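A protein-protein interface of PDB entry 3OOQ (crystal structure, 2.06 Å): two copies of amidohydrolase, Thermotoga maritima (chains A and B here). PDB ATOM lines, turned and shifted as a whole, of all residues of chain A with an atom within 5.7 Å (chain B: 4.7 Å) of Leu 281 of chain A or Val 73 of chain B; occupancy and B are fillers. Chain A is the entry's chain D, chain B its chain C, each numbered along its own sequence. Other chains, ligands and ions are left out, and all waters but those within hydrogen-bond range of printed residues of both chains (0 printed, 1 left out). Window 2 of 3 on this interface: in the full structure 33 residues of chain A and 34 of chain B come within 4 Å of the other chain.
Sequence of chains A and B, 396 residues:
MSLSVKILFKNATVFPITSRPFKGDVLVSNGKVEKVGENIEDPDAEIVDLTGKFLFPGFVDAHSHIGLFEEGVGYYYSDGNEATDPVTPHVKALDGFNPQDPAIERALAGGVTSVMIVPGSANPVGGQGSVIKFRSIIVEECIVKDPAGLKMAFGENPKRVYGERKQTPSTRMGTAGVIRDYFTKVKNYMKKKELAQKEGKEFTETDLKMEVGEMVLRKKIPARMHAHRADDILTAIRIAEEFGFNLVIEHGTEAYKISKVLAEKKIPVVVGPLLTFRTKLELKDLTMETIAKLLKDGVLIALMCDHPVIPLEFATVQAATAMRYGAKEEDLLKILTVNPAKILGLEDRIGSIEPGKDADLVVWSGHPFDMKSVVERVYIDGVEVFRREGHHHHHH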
ATOM      1  N   GLU A 156     -10.939   7.088   5.514  1.00  0.00           N
ATOM      2  CA  GLU A 156      -9.669   7.141   4.778  1.00  0.00           C
ATOM      3  C   GLU A 156      -8.831   8.396   5.010  1.00  0.00           C
ATOM      4  O   GLU A 156      -7.618   8.309   5.080  1.00  0.00           O
ATOM      5  CB  GLU A 156      -9.898   6.950   3.283  1.00  0.00           C
ATOM      6  CG  GLU A 156     -10.219   5.516   2.854  1.00  0.00           C
ATOM      7  CD  GLU A 156     -10.429   5.398   1.346  1.00  0.00           C
ATOM      8  OE1 GLU A 156      -9.711   6.086   0.578  1.00  0.00           O
ATOM      9  OE2 GLU A 156     -11.295   4.609   0.922  1.00  0.00           O
ATOM     10  N   ARG A 278     -16.368   9.367  -7.789  1.00  0.00           N
ATOM     11  CA  ARG A 278     -15.991   8.532  -6.639  1.00  0.00           C
ATOM     12  C   ARG A 278     -14.479   8.309  -6.632  1.00  0.00           C
ATOM     13  O   ARG A 278     -13.972   7.341  -7.188  1.00  0.00           O
ATOM     14  CB  ARG A 278     -16.780   7.215  -6.631  1.00  0.00           C
ATOM     15  CG  ARG A 278     -18.302   7.416  -6.589  1.00  0.00           C
ATOM     16  CD  ARG A 278     -19.014   6.188  -7.159  1.00  0.00           C
ATOM     17  NE  ARG A 278     -20.466   6.389  -7.245  1.00  0.00           N
ATOM     18  CZ  ARG A 278     -21.092   6.995  -8.259  1.00  0.00           C
ATOM     19  NH1 ARG A 278     -20.396   7.485  -9.283  1.00  0.00           N
ATOM     20  NH2 ARG A 278     -22.424   7.122  -8.248  1.00  0.00           N
ATOM     21  N   THR A 279     -13.772   9.250  -6.015  1.00  0.00           N
ATOM     22  CA  THR A 279     -12.316   9.296  -6.036  1.00  0.00           C
ATOM     23  C   THR A 279     -11.693   8.289  -5.096  1.00  0.00           C
ATOM     24  O   THR A 279     -10.497   8.067  -5.149  1.00  0.00           O
ATOM     25  CB  THR A 279     -11.796  10.683  -5.571  1.00  0.00           C
ATOM     26  OG1 THR A 279     -12.412  10.999  -4.312  1.00  0.00           O
ATOM     27  CG2 THR A 279     -12.100  11.780  -6.600  1.00  0.00           C
ATOM     28  N   LYS A 280     -12.474   7.728  -4.188  1.00  0.00           N
ATOM     29  CA  LYS A 280     -11.908   6.885  -3.154  1.00  0.00           C
ATOM     30  C   LYS A 280     -12.704   5.603  -3.017  1.00  0.00           C
ATOM     31  O   LYS A 280     -13.894   5.560  -3.339  1.00  0.00           O
ATOM     32  CB  LYS A 280     -11.881   7.635  -1.818  1.00  0.00           C
ATOM     33  CG  LYS A 280     -10.901   8.813  -1.757  1.00  0.00           C
ATOM     34  CD  LYS A 280     -10.980   9.501  -0.390  1.00  0.00           C
ATOM     35  CE  LYS A 280     -12.277  10.261  -0.199  1.00  0.00           C
ATOM     36  NZ  LYS A 280     -12.516  10.624   1.240  1.00  0.00           N
ATOM     37  N   LEU A 281     -12.035   4.567  -2.531  1.00  0.00           N
ATOM     38  CA  LEU A 281     -12.669   3.291  -2.189  1.00  0.00           C
ATOM     39  C   LEU A 281     -13.895   3.472  -1.298  1.00  0.00           C
ATOM     40  O   LEU A 281     -14.931   2.839  -1.520  1.00  0.00           O
ATOM     41  CB  LEU A 281     -11.645   2.389  -1.480  1.00  0.00           C
ATOM     42  CG  LEU A 281     -11.843   0.895  -1.271  1.00  0.00           C
ATOM     43  CD1 LEU A 281     -11.927   0.151  -2.616  1.00  0.00           C
ATOM     44  CD2 LEU A 281     -10.679   0.373  -0.406  1.00  0.00           C
ATOM     45  N   GLU A 282     -13.785   4.330  -0.285  1.00  0.00           N
ATOM     46  CA  GLU A 282     -14.928   4.576   0.620  1.00  0.00           C
ATOM     47  C   GLU A 282     -16.103   5.305  -0.057  1.00  0.00           C
ATOM     48  O   GLU A 282     -17.199   5.357   0.503  1.00  0.00           O
ATOM     49  CB  GLU A 282     -14.497   5.300   1.913  1.00  0.00           C
ATOM     50  CG  GLU A 282     -13.961   6.726   1.694  1.00  0.00           C
ATOM     51  CD  GLU A 282     -13.462   7.382   2.972  1.00  0.00           C
ATOM     52  OE1 GLU A 282     -13.483   6.744   4.035  1.00  0.00           O
ATOM     53  OE2 GLU A 282     -13.046   8.561   2.906  1.00  0.00           O
ATOM     54  N   LEU A 283     -15.890   5.816  -1.268  1.00  0.00           N
ATOM     55  CA  LEU A 283     -16.962   6.450  -2.053  1.00  0.00           C
ATOM     56  C   LEU A 283     -17.560   5.533  -3.108  1.00  0.00           C
ATOM     57  O   LEU A 283     -18.446   5.962  -3.847  1.00  0.00           O
ATOM     58  CB  LEU A 283     -16.473   7.751  -2.736  1.00  0.00           C
ATOM     59  CG  LEU A 283     -15.999   8.866  -1.803  1.00  0.00           C
ATOM     60  CD1 LEU A 283     -15.548  10.115  -2.576  1.00  0.00           C
ATOM     61  CD2 LEU A 283     -17.102   9.213  -0.839  1.00  0.00           C
ATOM     62  N   LYS A 284     -17.096   4.280  -3.183  1.00  0.00           N
ATOM     63  CA  LYS A 284     -17.524   3.388  -4.277  1.00  0.00           C
ATOM     64  C   LYS A 284     -19.053   3.225  -4.395  1.00  0.00           C
ATOM     65  O   LYS A 284     -19.567   3.042  -5.490  1.00  0.00           O
ATOM     66  CB  LYS A 284     -16.843   2.000  -4.199  1.00  0.00           C
ATOM     67  CG  LYS A 284     -17.365   1.077  -3.093  1.00  0.00           C
ATOM     68  CD  LYS A 284     -16.938  -0.410  -3.258  1.00  0.00           C
ATOM     69  CE  LYS A 284     -17.663  -1.277  -2.223  1.00  0.00           C
ATOM     70  NZ  LYS A 284     -17.152  -2.703  -2.120  1.00  0.00           N
ATOM     71  N   ASP A 285     -19.765   3.275  -3.274  1.00  0.00           N
ATOM     72  CA  ASP A 285     -21.222   3.075  -3.301  1.00  0.00           C
ATOM     73  C   ASP A 285     -22.007   4.369  -3.151  1.00  0.00           C
ATOM     74  O   ASP A 285     -23.206   4.352  -2.860  1.00  0.00           O
ATOM     75  CB  ASP A 285     -21.658   2.052  -2.246  1.00  0.00           C
ATOM     76  CG  ASP A 285     -21.302   0.618  -2.630  1.00  0.00           C
ATOM     77  OD1 ASP A 285     -21.037   0.338  -3.821  1.00  0.00           O
ATOM     78  OD2 ASP A 285     -21.288  -0.240  -1.727  1.00  0.00           O
ATOM     79  N   GLU B  70      -9.614   4.683 -12.711  1.00  0.00           N
ATOM     80  CA  GLU B  70     -10.736   3.803 -12.361  1.00  0.00           C
ATOM     81  C   GLU B  70     -11.583   4.426 -11.248  1.00  0.00           C
ATOM     82  O   GLU B  70     -11.047   5.013 -10.298  1.00  0.00           O
ATOM     83  CB  GLU B  70     -10.251   2.395 -11.962  1.00  0.00           C
ATOM     84  CG  GLU B  70     -11.401   1.411 -11.751  1.00  0.00           C
ATOM     85  CD  GLU B  70     -10.990   0.035 -11.206  1.00  0.00           C
ATOM     86  OE1 GLU B  70      -9.781  -0.297 -11.109  1.00  0.00           O
ATOM     87  OE2 GLU B  70     -11.902  -0.737 -10.864  1.00  0.00           O
ATOM     88  N   GLU B  71     -12.903   4.321 -11.373  1.00  0.00           N
ATOM     89  CA  GLU B  71     -13.785   4.891 -10.356  1.00  0.00           C
ATOM     90  C   GLU B  71     -13.942   3.991  -9.136  1.00  0.00           C
ATOM     91  O   GLU B  71     -14.027   2.780  -9.261  1.00  0.00           O
ATOM     92  CB  GLU B  71     -15.171   5.248 -10.930  1.00  0.00           C
ATOM     93  CG  GLU B  71     -15.997   6.083  -9.932  1.00  0.00           C
ATOM     94  CD  GLU B  71     -17.224   6.803 -10.527  1.00  0.00           C
ATOM     95  OE1 GLU B  71     -17.775   6.360 -11.565  1.00  0.00           O
ATOM     96  OE2 GLU B  71     -17.660   7.810  -9.913  1.00  0.00           O
ATOM     97  N   GLY B  72     -14.014   4.610  -7.960  1.00  0.00           N
ATOM     98  CA  GLY B  72     -14.345   3.921  -6.709  1.00  0.00           C
ATOM     99  C   GLY B  72     -13.196   3.123  -6.134  1.00  0.00           C
ATOM    100  O   GLY B  72     -13.406   2.096  -5.495  1.00  0.00           O
ATOM    101  N   VAL B  73     -11.977   3.623  -6.328  1.00  0.00           N
ATOM    102  CA  VAL B  73     -10.795   2.826  -6.092  1.00  0.00           C
ATOM    103  C   VAL B  73      -9.624   3.578  -5.397  1.00  0.00           C
ATOM    104  O   VAL B  73      -8.887   2.984  -4.593  1.00  0.00           O
ATOM    105  CB  VAL B  73     -10.445   2.161  -7.456  1.00  0.00           C
ATOM    106  CG1 VAL B  73      -9.105   2.572  -8.015  1.00  0.00           C
ATOM    107  CG2 VAL B  73     -10.735   0.709  -7.446  1.00  0.00           C
ATOM    108  N   GLY B  74      -9.476   4.871  -5.685  1.00  0.00           N
ATOM    109  CA  GLY B  74      -8.377   5.696  -5.141  1.00  0.00           C
ATOM    110  C   GLY B  74      -7.404   6.257  -6.183  1.00  0.00           C
ATOM    111  O   GLY B  74      -7.034   5.560  -7.130  1.00  0.00           O
ATOM    112  N   TYR B  77      -4.200   4.463  -7.962  1.00  0.00           N
ATOM    113  CA  TYR B  77      -4.359   3.471  -9.009  1.00  0.00           C
ATOM    114  C   TYR B  77      -4.553   4.051 -10.411  1.00  0.00           C
ATOM    115  O   TYR B  77      -4.782   3.297 -11.376  1.00  0.00           O
ATOM    116  CB  TYR B  77      -5.542   2.576  -8.664  1.00  0.00           C
ATOM    117  CG  TYR B  77      -5.303   1.680  -7.453  1.00  0.00           C
ATOM    118  CD1 TYR B  77      -4.322   0.670  -7.473  1.00  0.00           C
ATOM    119  CD2 TYR B  77      -6.079   1.817  -6.304  1.00  0.00           C
ATOM    120  CE1 TYR B  77      -4.110  -0.170  -6.353  1.00  0.00           C
ATOM    121  CE2 TYR B  77      -5.893   0.966  -5.182  1.00  0.00           C
ATOM    122  CZ  TYR B  77      -4.916  -0.014  -5.212  1.00  0.00           C
ATOM    123  OH  TYR B  77      -4.758  -0.834  -4.108  1.00  0.00           O
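The side-chain carboxylate (OE2) of Glu 71 of chain B is in salt-bridge range of the guanidinium group (NH1) of Arg 278 of chain A (2.8 Å).
N of Gly 72 of chain B lies within hydrogen-bond range of O of Arg 278 of chain A (2.8 Å).
N of Gly 74 of chain B lies close to O of Thr 279 of chain A (3.4 Å).
Of the printed residues of chain B, Arg 278 of chain A touches Glu 71 (2.8 Å) and Gly 72 (2.8 Å).
Of the printed residues of chain B, Thr 279 of chain A touches Gly 74 (3.2 Å).
Of the printed residues of chain B, Lys 280 of chain A touches Gly 72 and Val 73.
Leu 281 of chain A touches two residues of chain B.
Printed residues of chain A within 4 Å of Val 73 of chain B: Lys 280 (3.9 Å) and Leu 281 (3.9 Å).
Of the printed residues of chain A, Gly 74 of chain B touches Thr 279.
The nearest residue of chain B that does not touch Leu 281 of chain A is Gly 74 of chain B (4.1 Å).
The nearest printed residue of chain B that does not touch Lys 280 of chain A is Gly 74 of chain B (4.05 Å).
No position is printed for both chains.
Of the 8 pairs that touch across the chains among the printed residues, none has its exchanged pair printed and touching as well.
The side-chain amino group of Lys 280 of chain A is in salt-bridge range of the side-chain carboxylate of Glu 282 of chain A, 2.7 Å away.
Lys 280 of chain A touches Gly 72 of chain B (O to C, 3.8 Å).
C of Lys 280 of chain A touches N of Val 73 of chain B (3.9 Å).
Leu 281 of chain A touches Gly 72 of chain B.
Val 73 of chain B touches Leu 281 of chain A.
CB of Lys 284 of chain A touches O of Gly 72 of chain B, at 3.7 Å.
Hydrophobic or aromatic side chains of chain A within 4 Å of the printed part of chain B: Leu 281.
Of the 6 printed residues of chain B, 4 touch a printed residue of chain A.
Among the printed residues, 8 pairs touch across the chains.
Among the printed residues, Asp or Glu carboxylates within 4 Å of a Lys or Arg side-chain nitrogen of the other chain: Arg 278 of chain A with Glu 71 of chain B (2.8 Å).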
